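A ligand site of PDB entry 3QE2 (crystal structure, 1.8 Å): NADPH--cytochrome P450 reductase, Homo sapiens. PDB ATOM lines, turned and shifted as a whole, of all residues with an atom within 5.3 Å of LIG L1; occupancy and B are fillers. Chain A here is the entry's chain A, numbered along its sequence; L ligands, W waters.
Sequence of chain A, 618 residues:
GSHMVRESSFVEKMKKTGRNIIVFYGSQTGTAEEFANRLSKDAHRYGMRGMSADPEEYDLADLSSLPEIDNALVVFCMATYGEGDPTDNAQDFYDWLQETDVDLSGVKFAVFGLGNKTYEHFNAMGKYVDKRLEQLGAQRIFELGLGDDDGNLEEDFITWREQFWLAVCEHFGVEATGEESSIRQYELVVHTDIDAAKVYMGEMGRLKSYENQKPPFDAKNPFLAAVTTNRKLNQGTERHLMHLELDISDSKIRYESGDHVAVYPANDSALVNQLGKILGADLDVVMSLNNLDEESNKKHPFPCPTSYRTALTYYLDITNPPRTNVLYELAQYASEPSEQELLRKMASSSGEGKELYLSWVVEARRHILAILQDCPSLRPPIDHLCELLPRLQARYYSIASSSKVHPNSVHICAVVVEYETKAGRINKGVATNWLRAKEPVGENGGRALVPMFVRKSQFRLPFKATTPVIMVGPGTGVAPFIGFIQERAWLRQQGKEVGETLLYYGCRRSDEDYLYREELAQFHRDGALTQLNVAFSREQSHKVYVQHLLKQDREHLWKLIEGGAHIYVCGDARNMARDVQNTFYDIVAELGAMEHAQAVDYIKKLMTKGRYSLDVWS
The backbone NH (N) of Thr 31 sits at hydrogen-bond distance from the side-chain hydroxyl (OG) of Ser 27 (3.4 Å).
The backbone NH (N) of Ser 27 sits at hydrogen-bond distance from the side-chain hydroxyl (OG1) of Thr 87, 3.4 Å away.
O of Leu 114 is in hydrogen-bond range of N of Thr 80 (3.1 Å).
N of Ala 124 is in hydrogen-bond range of OG1 of Thr 80 (3.2 Å).
The side-chain amide nitrogen (NE2) of Gln 28 sits at hydrogen-bond distance from the side-chain hydroxyl (OH) of Tyr 396 (2.8 Å).
The backbone NH (N) of Gly 115 lies close to the side-chain amide nitrogen (ND2) of Asn 123 (3.3 Å).
The side-chain amide nitrogen (ND2) of Asn 123 sits close to the backbone NH (N) of Leu 114 (3.1 Å).
The backbone NH of Ala 79 sits at hydrogen-bond distance from the backbone carbonyl oxygen of Gly 26.
Gly 30 touches LIG L1 (N to O7, 3.5 Å).
Ala 79 touches LIG L1 (CB to O6, 3.3 Å).
Gly 82 touches LIG L1.
Gly 115 touches LIG L1 (CA to O1, 3.2 Å).
Tyr 119 touches LIG L1.
Phe 122 touches LIG L1 (CA to O1, 3.3 Å).
Asp 149 touches LIG L1 (OD1 to O4, 3.8 Å).
Leu 153 touches LIG L1 (CD2 to O5, 3.5 Å).
Hydrophobic or aromatic side chains within 4 Å of LIG L1: Ala 32, Ala 79, Tyr 81, Leu 114, Tyr 119, Phe 122 and Leu 153.
Of the 28 residues printed, 20 come within 4 Å of LIG L1.
The nearest printed residue that does not touch LIG L1 is Glu 83 (4.1 Å).
Water W1 lies within hydrogen-bond range of OD1 of Asp 149 (2.7 Å), O4 of LIG L1 (2.7 Å) and ND2 of Asn 116 (3.0 Å).
Water W4 lies within hydrogen-bond range of an oxygen (O2) of LIG L1 (2.7 Å), the backbone NH of His 121 (2.9 Å) and the backbone NH of Glu 120 (3.3 Å).
Water W3 bridges OG1 of Thr 31 and O5 of LIG L1.
Water W5 lies within hydrogen-bond range of N of Glu 83 and N3 of LIG L1.
O9 of LIG L1 lies within hydrogen-bond range of OG of Ser 27, at 2.5 Å.
O8 of LIG L1 sits at hydrogen-bond distance from N of Thr 29.
An oxygen (O7) of LIG L1 sits at hydrogen-bond distance from the side-chain hydroxyl (OG1) of Thr 29 (2.5 Å).
An oxygen (O3) of LIG L1 is in hydrogen-bond range of the backbone NH of Thr 80.
An oxygen (O3) of LIG L1 sits at hydrogen-bond distance from the backbone carbonyl oxygen (O) of Thr 80 (2.6 Å).
The side-chain hydroxyl (OH) of Tyr 81 sits at hydrogen-bond distance from an oxygen (O8) of LIG L1.
N of Thr 31 sits at hydrogen-bond distance from O7 of LIG L1 (2.9 Å).
An oxygen (O7) of LIG L1 lies within hydrogen-bond range of the side-chain hydroxyl (OG1) of Thr 31, at 2.7 Å.
The backbone NH (N) of Gln 28 lies within hydrogen-bond range of an oxygen (O8) of LIG L1, 2.7 Å away.
The backbone NH of Asn 123 lies within hydrogen-bond range of an oxygen (O1) of LIG L1 (2.7 Å).
N of Ala 32 sits at hydrogen-bond distance from O9 of LIG L1 (2.8 Å).
O of His 121 lies within hydrogen-bond range of N2 of LIG L1, at 2.9 Å.
An oxygen (O1) of LIG L1 lies within hydrogen-bond range of the backbone NH of Asn 116 (2.9 Å).
The backbone carbonyl oxygen of Leu 114 is in hydrogen-bond range of an oxygen (O3) of LIG L1.
N of Gly 84 lies within hydrogen-bond range of O2 of LIG L1.
The backbone NH (N) of Tyr 396 is in hydrogen-bond range of an oxygen (O9) of LG2 L2, 3.3 Å away.
O9 of LG2 L2 lies within hydrogen-bond range of O of Tyr 396 (2.6 Å).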
ATOM      1  N   GLY A  26      15.980   6.343  19.158  1.00  0.00           N
ATOM      2  CA  GLY A  26      16.430   5.170  18.432  1.00  0.00           C
ATOM      3  C   GLY A  26      17.654   4.796  19.233  1.00  0.00           C
ATOM      4  O   GLY A  26      18.710   5.424  19.090  1.00  0.00           O
ATOM      5  N   SER A  27      17.540   3.773  20.085  1.00  0.00           N
ATOM      6  CA  SER A  27      18.634   3.406  20.967  1.00  0.00           C
ATOM      7  C   SER A  27      18.828   1.900  21.109  1.00  0.00           C
ATOM      8  O   SER A  27      17.867   1.138  21.069  1.00  0.00           O
ATOM      9  CB  SER A  27      18.344   4.011  22.358  1.00  0.00           C
ATOM     10  OG  SER A  27      19.440   3.885  23.257  1.00  0.00           O
ATOM     11  N   GLN A  28      20.080   1.480  21.260  1.00  0.00           N
ATOM     12  CA  GLN A  28      20.406   0.066  21.448  1.00  0.00           C
ATOM     13  C   GLN A  28      20.988  -0.114  22.841  1.00  0.00           C
ATOM     14  O   GLN A  28      20.621  -1.051  23.552  1.00  0.00           O
ATOM     15  CB  GLN A  28      21.388  -0.426  20.388  1.00  0.00           C
ATOM     16  CG  GLN A  28      21.654  -1.926  20.475  1.00  0.00           C
ATOM     17  CD  GLN A  28      22.482  -2.457  19.312  1.00  0.00           C
ATOM     18  OE1 GLN A  28      22.071  -2.380  18.148  1.00  0.00           O
ATOM     19  NE2 GLN A  28      23.651  -3.013  19.615  1.00  0.00           N
ATOM     20  N   THR A  29      21.890   0.778  23.262  1.00  0.00           N
ATOM     21  CA  THR A  29      22.457   0.669  24.592  1.00  0.00           C
ATOM     22  C   THR A  29      22.064   1.807  25.525  1.00  0.00           C
ATOM     23  O   THR A  29      22.823   2.202  26.419  1.00  0.00           O
ATOM     24  CB  THR A  29      24.008   0.514  24.562  1.00  0.00           C
ATOM     25  OG1 THR A  29      24.599   1.675  23.972  1.00  0.00           O
ATOM     26  CG2 THR A  29      24.392  -0.725  23.756  1.00  0.00           C
ATOM     27  N   GLY A  30      20.862   2.334  25.306  1.00  0.00           N
ATOM     28  CA  GLY A  30      20.308   3.362  26.176  1.00  0.00           C
ATOM     29  C   GLY A  30      20.731   4.818  26.164  1.00  0.00           C
ATOM     30  O   GLY A  30      20.118   5.621  26.869  1.00  0.00           O
ATOM     31  N   THR A  31      21.760   5.193  25.396  1.00  0.00           N
ATOM     32  CA  THR A  31      22.215   6.578  25.405  1.00  0.00           C
ATOM     33  C   THR A  31      21.184   7.529  24.791  1.00  0.00           C
ATOM     34  O   THR A  31      20.902   8.583  25.351  1.00  0.00           O
ATOM     35  CB  THR A  31      23.542   6.744  24.629  1.00  0.00           C
ATOM     36  OG1 THR A  31      24.446   5.712  25.027  1.00  0.00           O
ATOM     37  CG2 THR A  31      24.163   8.085  24.947  1.00  0.00           C
ATOM     38  N   ALA A  32      20.639   7.153  23.641  1.00  0.00           N
ATOM     39  CA  ALA A  32      19.646   7.993  22.970  1.00  0.00           C
ATOM     40  C   ALA A  32      18.388   8.092  23.835  1.00  0.00           C
ATOM     41  O   ALA A  32      17.751   9.153  23.905  1.00  0.00           O
ATOM     42  CB  ALA A  32      19.313   7.416  21.591  1.00  0.00           C
ATOM     43  N   GLU A  33      18.034   6.996  24.496  1.00  0.00           N
ATOM     44  CA  GLU A  33      16.850   7.020  25.356  1.00  0.00           C
ATOM     45  C   GLU A  33      17.052   8.019  26.487  1.00  0.00           C
ATOM     46  O   GLU A  33      16.139   8.763  26.836  1.00  0.00           O
ATOM     47  CB  GLU A  33      16.543   5.641  25.937  1.00  0.00           C
ATOM     48  CG  GLU A  33      15.357   5.674  26.910  1.00  0.00           C
ATOM     49  CD  GLU A  33      14.954   4.311  27.433  1.00  0.00           C
ATOM     50  OE1 GLU A  33      13.986   4.233  28.219  1.00  0.00           O
ATOM     51  OE2 GLU A  33      15.611   3.313  27.060  1.00  0.00           O
ATOM     52  N   ALA A  79      20.399   6.941  17.238  1.00  0.00           N
ATOM     53  CA  ALA A  79      21.749   6.407  17.164  1.00  0.00           C
ATOM     54  C   ALA A  79      21.864   5.631  15.859  1.00  0.00           C
ATOM     55  O   ALA A  79      20.893   5.085  15.362  1.00  0.00           O
ATOM     56  CB  ALA A  79      22.015   5.477  18.338  1.00  0.00           C
ATOM     57  N   THR A  80      23.081   5.601  15.312  1.00  0.00           N
ATOM     58  CA  THR A  80      23.345   4.866  14.075  1.00  0.00           C
ATOM     59  C   THR A  80      24.121   3.592  14.425  1.00  0.00           C
ATOM     60  O   THR A  80      25.030   3.628  15.250  1.00  0.00           O
ATOM     61  CB  THR A  80      24.195   5.715  13.108  1.00  0.00           C
ATOM     62  OG1 THR A  80      23.471   6.885  12.716  1.00  0.00           O
ATOM     63  CG2 THR A  80      24.554   4.903  11.859  1.00  0.00           C
ATOM     64  N   TYR A  81      23.749   2.479  13.805  1.00  0.00           N
ATOM     65  CA  TYR A  81      24.458   1.220  14.054  1.00  0.00           C
ATOM     66  C   TYR A  81      24.984   0.579  12.769  1.00  0.00           C
ATOM     67  O   TYR A  81      25.052   1.226  11.729  1.00  0.00           O
ATOM     68  CB  TYR A  81      23.576   0.245  14.836  1.00  0.00           C
ATOM     69  CG  TYR A  81      23.699   0.463  16.320  1.00  0.00           C
ATOM     70  CD1 TYR A  81      23.121   1.575  16.943  1.00  0.00           C
ATOM     71  CD2 TYR A  81      24.475  -0.394  17.112  1.00  0.00           C
ATOM     72  CE1 TYR A  81      23.321   1.840  18.301  1.00  0.00           C
ATOM     73  CE2 TYR A  81      24.689  -0.140  18.471  1.00  0.00           C
ATOM     74  CZ  TYR A  81      24.112   0.982  19.051  1.00  0.00           C
ATOM     75  OH  TYR A  81      24.341   1.245  20.383  1.00  0.00           O
ATOM     76  N   GLY A  82      25.356  -0.687  12.868  1.00  0.00           N
ATOM     77  CA  GLY A  82      25.915  -1.422  11.738  1.00  0.00           C
ATOM     78  C   GLY A  82      25.687  -0.903  10.335  1.00  0.00           C
ATOM     79  O   GLY A  82      24.573  -0.910   9.831  1.00  0.00           O
ATOM     80  N   GLU A  83      26.760  -0.442   9.696  1.00  0.00           N
ATOM     81  CA  GLU A  83      26.699   0.036   8.312  1.00  0.00           C
ATOM     82  C   GLU A  83      25.751   1.219   8.062  1.00  0.00           C
ATOM     83  O   GLU A  83      25.179   1.356   6.973  1.00  0.00           O
ATOM     84  CB  GLU A  83      26.333  -1.124   7.380  1.00  0.00           C
ATOM     85  CG  GLU A  83      27.276  -2.336   7.438  1.00  0.00           C
ATOM     86  CD  GLU A  83      27.003  -3.262   8.626  1.00  0.00           C
ATOM     87  OE1 GLU A  83      27.885  -3.406   9.504  1.00  0.00           O
ATOM     88  OE2 GLU A  83      25.902  -3.866   8.662  1.00  0.00           O
ATOM     89  N   GLY A  84      25.593   2.071   9.070  1.00  0.00           N
ATOM     90  CA  GLY A  84      24.727   3.238   8.935  1.00  0.00           C
ATOM     91  C   GLY A  84      23.259   2.897   8.964  1.00  0.00           C
ATOM     92  O   GLY A  84      22.440   3.615   8.381  1.00  0.00           O
ATOM     93  N   THR A  87      18.675   1.592  14.644  1.00  0.00           N
ATOM     94  CA  THR A  87      18.659   0.660  15.753  1.00  0.00           C
ATOM     95  C   THR A  87      17.441  -0.234  15.508  1.00  0.00           C
ATOM     96  O   THR A  87      16.556   0.139  14.730  1.00  0.00           O
ATOM     97  CB  THR A  87      18.479   1.410  17.092  1.00  0.00           C
ATOM     98  OG1 THR A  87      17.376   2.321  16.984  1.00  0.00           O
ATOM     99  CG2 THR A  87      19.737   2.190  17.429  1.00  0.00           C
ATOM    100  N   LEU A 114      23.148  10.478  17.264  1.00  0.00           N
ATOM    101  CA  LEU A 114      24.226   9.932  18.081  1.00  0.00           C
ATOM    102  C   LEU A 114      25.019   9.051  17.133  1.00  0.00           C
ATOM    103  O   LEU A 114      24.454   8.140  16.516  1.00  0.00           O
ATOM    104  CB  LEU A 114      23.688   9.062  19.219  1.00  0.00           C
ATOM    105  CG  LEU A 114      22.951   9.768  20.351  1.00  0.00           C
ATOM    106  CD1 LEU A 114      21.565  10.199  19.899  1.00  0.00           C
ATOM    107  CD2 LEU A 114      22.867   8.800  21.522  1.00  0.00           C
ATOM    108  N   GLY A 115      26.307   9.323  17.021  1.00  0.00           N
ATOM    109  CA  GLY A 115      27.139   8.529  16.139  1.00  0.00           C
ATOM    110  C   GLY A 115      28.568   8.476  16.630  1.00  0.00           C
ATOM    111  O   GLY A 115      28.856   8.807  17.786  1.00  0.00           O
ATOM    112  N   ASN A 116      29.473   8.067  15.760  1.00  0.00           N
ATOM    113  CA  ASN A 116      30.882   7.977  16.130  1.00  0.00           C
ATOM    114  C   ASN A 116      31.655   8.102  14.815  1.00  0.00           C
ATOM    115  O   ASN A 116      31.473   7.291  13.912  1.00  0.00           O
ATOM    116  CB  ASN A 116      31.134   6.612  16.790  1.00  0.00           C
ATOM    117  CG  ASN A 116      32.585   6.408  17.182  1.00  0.00           C
ATOM    118  OD1 ASN A 116      33.490   6.731  16.416  1.00  0.00           O
ATOM    119  ND2 ASN A 116      32.811   5.862  18.365  1.00  0.00           N
ATOM    120  N   LYS A 117      32.494   9.123  14.711  1.00  0.00           N
ATOM    121  CA  LYS A 117      33.243   9.370  13.481  1.00  0.00           C
ATOM    122  C   LYS A 117      34.252   8.310  13.047  1.00  0.00           C
ATOM    123  O   LYS A 117      34.784   8.418  11.945  1.00  0.00           O
ATOM    124  CB  LYS A 117      33.929  10.740  13.532  1.00  0.00           C
ATOM    125  CG  LYS A 117      32.947  11.903  13.480  1.00  0.00           C
ATOM    126  CD  LYS A 117      33.633  13.226  13.156  1.00  0.00           C
ATOM    127  CE  LYS A 117      34.580  13.658  14.260  1.00  0.00           C
ATOM    128  NZ  LYS A 117      35.083  15.042  14.044  1.00  0.00           N
ATOM    129  N   TYR A 119      33.496   5.337  12.416  1.00  0.00           N
ATOM    130  CA  TYR A 119      32.746   4.430  11.560  1.00  0.00           C
ATOM    131  C   TYR A 119      32.600   5.014  10.153  1.00  0.00           C
ATOM    132  O   TYR A 119      32.715   6.211   9.961  1.00  0.00           O
ATOM    133  CB  TYR A 119      31.367   4.168  12.172  1.00  0.00           C
ATOM    134  CG  TYR A 119      31.416   3.301  13.404  1.00  0.00           C
ATOM    135  CD1 TYR A 119      31.495   1.915  13.303  1.00  0.00           C
ATOM    136  CD2 TYR A 119      31.410   3.870  14.674  1.00  0.00           C
ATOM    137  CE1 TYR A 119      31.571   1.107  14.444  1.00  0.00           C
ATOM    138  CE2 TYR A 119      31.479   3.083  15.823  1.00  0.00           C
ATOM    139  CZ  TYR A 119      31.560   1.707  15.694  1.00  0.00           C
ATOM    140  OH  TYR A 119      31.638   0.920  16.821  1.00  0.00           O
ATOM    141  N   GLU A 120      32.332   4.148   9.177  1.00  0.00           N
ATOM    142  CA  GLU A 120      32.175   4.582   7.797  1.00  0.00           C
ATOM    143  C   GLU A 120      30.993   5.519   7.532  1.00  0.00           C
ATOM    144  O   GLU A 120      31.117   6.511   6.808  1.00  0.00           O
ATOM    145  CB  GLU A 120      32.055   3.376   6.864  1.00  0.00           C
ATOM    146  CG  GLU A 120      33.376   2.869   6.337  1.00  0.00           C
ATOM    147  CD  GLU A 120      34.094   3.905   5.495  1.00  0.00           C
ATOM    148  OE1 GLU A 120      33.538   4.320   4.450  1.00  0.00           O
ATOM    149  OE2 GLU A 120      35.208   4.313   5.875  1.00  0.00           O
ATOM    150  N   HIS A 121      29.845   5.194   8.114  1.00  0.00           N
ATOM    151  CA  HIS A 121      28.639   5.992   7.904  1.00  0.00           C
ATOM    152  C   HIS A 121      28.321   6.781   9.168  1.00  0.00           C
ATOM    153  O   HIS A 121      27.442   6.417   9.933  1.00  0.00           O
ATOM    154  CB  HIS A 121      27.492   5.064   7.547  1.00  0.00           C
ATOM    155  CG  HIS A 121      27.776   4.217   6.338  1.00  0.00           C
ATOM    156  ND1 HIS A 121      27.670   4.697   5.051  1.00  0.00           N
ATOM    157  CD2 HIS A 121      28.217   2.938   6.233  1.00  0.00           C
ATOM    158  CE1 HIS A 121      28.038   3.751   4.198  1.00  0.00           C
ATOM    159  NE2 HIS A 121      28.378   2.671   4.891  1.00  0.00           N
ATOM    160  N   PHE A 122      29.050   7.876   9.366  1.00  0.00           N
ATOM    161  CA  PHE A 122      28.886   8.706  10.543  1.00  0.00           C
ATOM    162  C   PHE A 122      27.513   9.351  10.645  1.00  0.00           C
ATOM    163  O   PHE A 122      27.124  10.135   9.785  1.00  0.00           O
ATOM    164  CB  PHE A 122      29.952   9.792  10.559  1.00  0.00           C
ATOM    165  CG  PHE A 122      29.786  10.784  11.666  1.00  0.00           C
ATOM    166  CD1 PHE A 122      29.782  10.370  12.993  1.00  0.00           C
ATOM    167  CD2 PHE A 122      29.650  12.137  11.391  1.00  0.00           C
ATOM    168  CE1 PHE A 122      29.620  11.292  14.036  1.00  0.00           C
ATOM    169  CE2 PHE A 122      29.483  13.069  12.412  1.00  0.00           C
ATOM    170  CZ  PHE A 122      29.478  12.646  13.739  1.00  0.00           C
ATOM    171  N   ASN A 123      26.790   9.005  11.719  1.00  0.00           N
ATOM    172  CA  ASN A 123      25.478   9.564  11.993  1.00  0.00           C
ATOM    173  C   ASN A 123      24.508   9.425  10.819  1.00  0.00           C
ATOM    174  O   ASN A 123      23.630  10.263  10.618  1.00  0.00           O
ATOM    175  CB  ASN A 123      25.615  11.034  12.390  1.00  0.00           C
ATOM    176  CG  ASN A 123      25.538  11.245  13.897  1.00  0.00           C
ATOM    177  OD1 ASN A 123      26.334  11.981  14.476  1.00  0.00           O
ATOM    178  ND2 ASN A 123      24.574  10.597  14.530  1.00  0.00           N
ATOM    179  N   ALA A 124      24.659   8.341  10.065  1.00  0.00           N
ATOM    180  CA  ALA A 124      23.803   8.105   8.915  1.00  0.00           C
ATOM    181  C   ALA A 124      22.308   8.134   9.242  1.00  0.00           C
ATOM    182  O   ALA A 124      21.511   8.662   8.447  1.00  0.00           O
ATOM    183  CB  ALA A 124      24.169   6.766   8.270  1.00  0.00           C
ATOM    184  N   ASP A 149      30.593  10.255  19.550  1.00  0.00           N
ATOM    185  CA  ASP A 149      31.090   9.522  20.711  1.00  0.00           C
ATOM    186  C   ASP A 149      32.595   9.309  20.665  1.00  0.00           C
ATOM    187  O   ASP A 149      33.193   8.852  21.639  1.00  0.00           O
ATOM    188  CB  ASP A 149      30.379   8.162  20.822  1.00  0.00           C
ATOM    189  CG  ASP A 149      30.600   7.504  22.180  1.00  0.00           C
ATOM    190  OD1 ASP A 149      30.806   6.268  22.218  1.00  0.00           O
ATOM    191  OD2 ASP A 149      30.553   8.208  23.211  1.00  0.00           O
ATOM    192  N   LEU A 153      30.462  12.871  23.367  1.00  0.00           N
ATOM    193  CA  LEU A 153      29.057  12.912  22.989  1.00  0.00           C
ATOM    194  C   LEU A 153      28.238  13.805  23.922  1.00  0.00           C
ATOM    195  O   LEU A 153      27.368  14.564  23.473  1.00  0.00           O
ATOM    196  CB  LEU A 153      28.495  11.494  22.984  1.00  0.00           C
ATOM    197  CG  LEU A 153      27.051  11.327  22.519  1.00  0.00           C
ATOM    198  CD1 LEU A 153      26.912  11.911  21.105  1.00  0.00           C
ATOM    199  CD2 LEU A 153      26.668   9.847  22.546  1.00  0.00           C
ATOM    200  N   TYR A 396      29.509  -6.454  23.968  1.00  0.00           N
ATOM    201  CA  TYR A 396      29.529  -7.325  22.787  1.00  0.00           C
ATOM    202  C   TYR A 396      30.925  -7.890  22.516  1.00  0.00           C
ATOM    203  O   TYR A 396      31.926  -7.212  22.705  1.00  0.00           O
ATOM    204  CB  TYR A 396      29.092  -6.544  21.558  1.00  0.00           C
ATOM    205  CG  TYR A 396      27.740  -5.891  21.697  1.00  0.00           C
ATOM    206  CD1 TYR A 396      26.584  -6.662  21.786  1.00  0.00           C
ATOM    207  CD2 TYR A 396      27.618  -4.512  21.768  1.00  0.00           C
ATOM    208  CE1 TYR A 396      25.334  -6.065  21.948  1.00  0.00           C
ATOM    209  CE2 TYR A 396      26.369  -3.905  21.930  1.00  0.00           C
ATOM    210  CZ  TYR A 396      25.233  -4.697  22.013  1.00  0.00           C
ATOM    211  OH  TYR A 396      23.996  -4.111  22.190  1.00  0.00           O
HETATM  212  N1  LIG L   1      28.048   5.460  14.752  1.00  0.00           N
HETATM  213  C1  LIG L   1      28.014   5.976  13.496  1.00  0.00           C
HETATM  214  O1  LIG L   1      28.051   7.187  13.337  1.00  0.00           O
HETATM  215  N2  LIG L   1      27.926   5.120  12.433  1.00  0.00           N
HETATM  216  C2  LIG L   1      27.886   3.719  12.526  1.00  0.00           C
HETATM  217  O2  LIG L   1      27.808   3.143  11.444  1.00  0.00           O
HETATM  218  C3  LIG L   1      27.935   3.141  13.860  1.00  0.00           C
HETATM  219  N3  LIG L   1      27.908   1.739  13.982  1.00  0.00           N
HETATM  220  C4  LIG L   1      27.965   1.262  15.274  1.00  0.00           C
HETATM  221  C5  LIG L   1      27.943  -0.181  15.403  1.00  0.00           C
HETATM  222  C6  LIG L   1      28.005  -0.818  16.652  1.00  0.00           C
HETATM  223  C7  LIG L   1      27.988  -2.360  16.632  1.00  0.00           C
HETATM  224  C8  LIG L   1      28.092  -0.014  17.906  1.00  0.00           C
HETATM  225  C9  LIG L   1      28.159  -0.613  19.332  1.00  0.00           C
HETATM  226  C10 LIG L   1      28.110   1.368  17.805  1.00  0.00           C
HETATM  227  C11 LIG L   1      28.046   2.066  16.507  1.00  0.00           C
HETATM  228  N4  LIG L   1      28.072   3.540  16.307  1.00  0.00           N
HETATM  229  C12 LIG L   1      28.015   4.098  14.938  1.00  0.00           C
HETATM  230  C13 LIG L   1      28.144   4.396  17.455  1.00  0.00           C
HETATM  231  C14 LIG L   1      26.780   4.653  18.170  1.00  0.00           C
HETATM  232  O3  LIG L   1      25.817   5.173  17.229  1.00  0.00           O
HETATM  233  C15 LIG L   1      26.995   5.550  19.379  1.00  0.00           C
HETATM  234  O4  LIG L   1      27.846   4.797  20.287  1.00  0.00           O
HETATM  235  C16 LIG L   1      25.621   5.859  20.066  1.00  0.00           C
HETATM  236  O5  LIG L   1      25.979   6.737  21.193  1.00  0.00           O
HETATM  237  C17 LIG L   1      24.929   4.653  20.638  1.00  0.00           C
HETATM  238  O6  LIG L   1      23.618   5.009  21.200  1.00  0.00           O
HETATM  239  P1  LIG L   1      22.749   4.063  22.067  1.00  0.00           P
HETATM  240  O7  LIG L   1      23.395   3.849  23.413  1.00  0.00           O
HETATM  241  O8  LIG L   1      22.402   2.829  21.333  1.00  0.00           O
HETATM  242  O9  LIG L   1      21.533   4.887  22.296  1.00  0.00           O
HETATM  243  P1  LG2 L   2      34.364  -1.098  30.602  1.00  0.00           P
HETATM  244  O1  LG2 L   2      34.096  -1.136  32.080  1.00  0.00           O
HETATM  245  O2  LG2 L   2      33.200  -0.807  29.738  1.00  0.00           O
HETATM  246  O3  LG2 L   2      35.392  -0.037  30.391  1.00  0.00           O
HETATM  247  C1  LG2 L   2      35.904   0.335  29.078  1.00  0.00           C
HETATM  248  C2  LG2 L   2      36.350   1.791  29.003  1.00  0.00           C
HETATM  249  O4  LG2 L   2      37.501   1.962  29.856  1.00  0.00           O
HETATM  250  C3  LG2 L   2      36.870   2.263  27.634  1.00  0.00           C
HETATM  251  O5  LG2 L   2      35.806   2.688  26.795  1.00  0.00           O
HETATM  252  C4  LG2 L   2      37.688   3.501  28.006  1.00  0.00           C
HETATM  253  O6  LG2 L   2      36.944   4.748  28.229  1.00  0.00           O
HETATM  254  C5  LG2 L   2      38.338   3.008  29.314  1.00  0.00           C
HETATM  255  N1  LG2 L   2      39.751   2.541  29.200  1.00  0.00           N
HETATM  256  C6  LG2 L   2      40.328   1.316  28.887  1.00  0.00           C
HETATM  257  N2  LG2 L   2      41.710   1.320  28.917  1.00  0.00           N
HETATM  258  C7  LG2 L   2      42.014   2.610  29.269  1.00  0.00           C
HETATM  259  C8  LG2 L   2      43.245   3.354  29.492  1.00  0.00           C
HETATM  260  N3  LG2 L   2      44.481   2.777  29.372  1.00  0.00           N
HETATM  261  N4  LG2 L   2      43.085   4.693  29.845  1.00  0.00           N
HETATM  262  C9  LG2 L   2      41.926   5.384  29.996  1.00  0.00           C
HETATM  263  N5  LG2 L   2      40.704   4.790  29.817  1.00  0.00           N
HETATM  264  C10 LG2 L   2      40.804   3.395  29.447  1.00  0.00           C
HETATM  265  N6  LG2 L   2      36.521  -6.778  23.087  1.00  0.00           N
HETATM  266  C11 LG2 L   2      37.302  -7.899  23.099  1.00  0.00           C
HETATM  267  O7  LG2 L   2      38.166  -8.001  23.956  1.00  0.00           O
HETATM  268  N7  LG2 L   2      37.056  -8.836  22.151  1.00  0.00           N
HETATM  269  C12 LG2 L   2      36.079  -8.806  21.120  1.00  0.00           C
HETATM  270  O8  LG2 L   2      35.971  -9.743  20.332  1.00  0.00           O
HETATM  271  C13 LG2 L   2      35.269  -7.593  21.101  1.00  0.00           C
HETATM  272  N8  LG2 L   2      34.301  -7.513  20.093  1.00  0.00           N
HETATM  273  C14 LG2 L   2      33.538  -6.344  20.096  1.00  0.00           C
HETATM  274  C15 LG2 L   2      32.532  -6.211  19.044  1.00  0.00           C
HETATM  275  C16 LG2 L   2      31.699  -5.067  18.946  1.00  0.00           C
HETATM  276  C17 LG2 L   2      30.651  -4.961  17.822  1.00  0.00           C
HETATM  277  C18 LG2 L   2      31.873  -3.995  19.956  1.00  0.00           C
HETATM  278  C19 LG2 L   2      31.038  -2.711  19.966  1.00  0.00           C
HETATM  279  C20 LG2 L   2      32.818  -4.094  20.972  1.00  0.00           C
HETATM  280  C21 LG2 L   2      33.679  -5.240  21.085  1.00  0.00           C
HETATM  281  N9  LG2 L   2      34.724  -5.425  22.123  1.00  0.00           N
HETATM  282  C22 LG2 L   2      35.524  -6.587  22.128  1.00  0.00           C
HETATM  283  C23 LG2 L   2      34.998  -4.441  23.214  1.00  0.00           C
HETATM  284  C24 LG2 L   2      33.958  -5.099  24.277  1.00  0.00           C
HETATM  285  O9  LG2 L   2      32.511  -5.036  23.927  1.00  0.00           O
HETATM  286  C25 LG2 L   2      34.102  -4.239  25.631  1.00  0.00           C
HETATM  287  O10 LG2 L   2      33.964  -2.805  25.392  1.00  0.00           O
HETATM  288  C26 LG2 L   2      35.447  -4.420  26.360  1.00  0.00           C
HETATM  289  O11 LG2 L   2      35.601  -5.834  26.600  1.00  0.00           O
HETATM  290  C27 LG2 L   2      35.537  -3.696  27.606  1.00  0.00           C
HETATM  291  O12 LG2 L   2      34.432  -3.867  28.501  1.00  0.00           O
HETATM  292  P2  LG2 L   2      34.533  -3.778  29.997  1.00  0.00           P
HETATM  293  O13 LG2 L   2      35.483  -4.774  30.588  1.00  0.00           O
HETATM  294  O14 LG2 L   2      33.126  -3.966  30.474  1.00  0.00           O
HETATM  295  O15 LG2 L   2      35.110  -2.311  30.103  1.00  0.00           O
HETATM  296  O   HOH W   1      30.557   4.742  20.020  1.00  0.00           O
HETATM  297  O   HOH W   2      25.721  -2.959  14.394  1.00  0.00           O
HETATM  298  O   HOH W   3      26.878   5.875  23.757  1.00  0.00           O
HETATM  299  O   HOH W   4      29.409   2.554   9.297  1.00  0.00           O
HETATM  300  O   HOH W   5      28.763   0.045  11.735  1.00  0.00           O
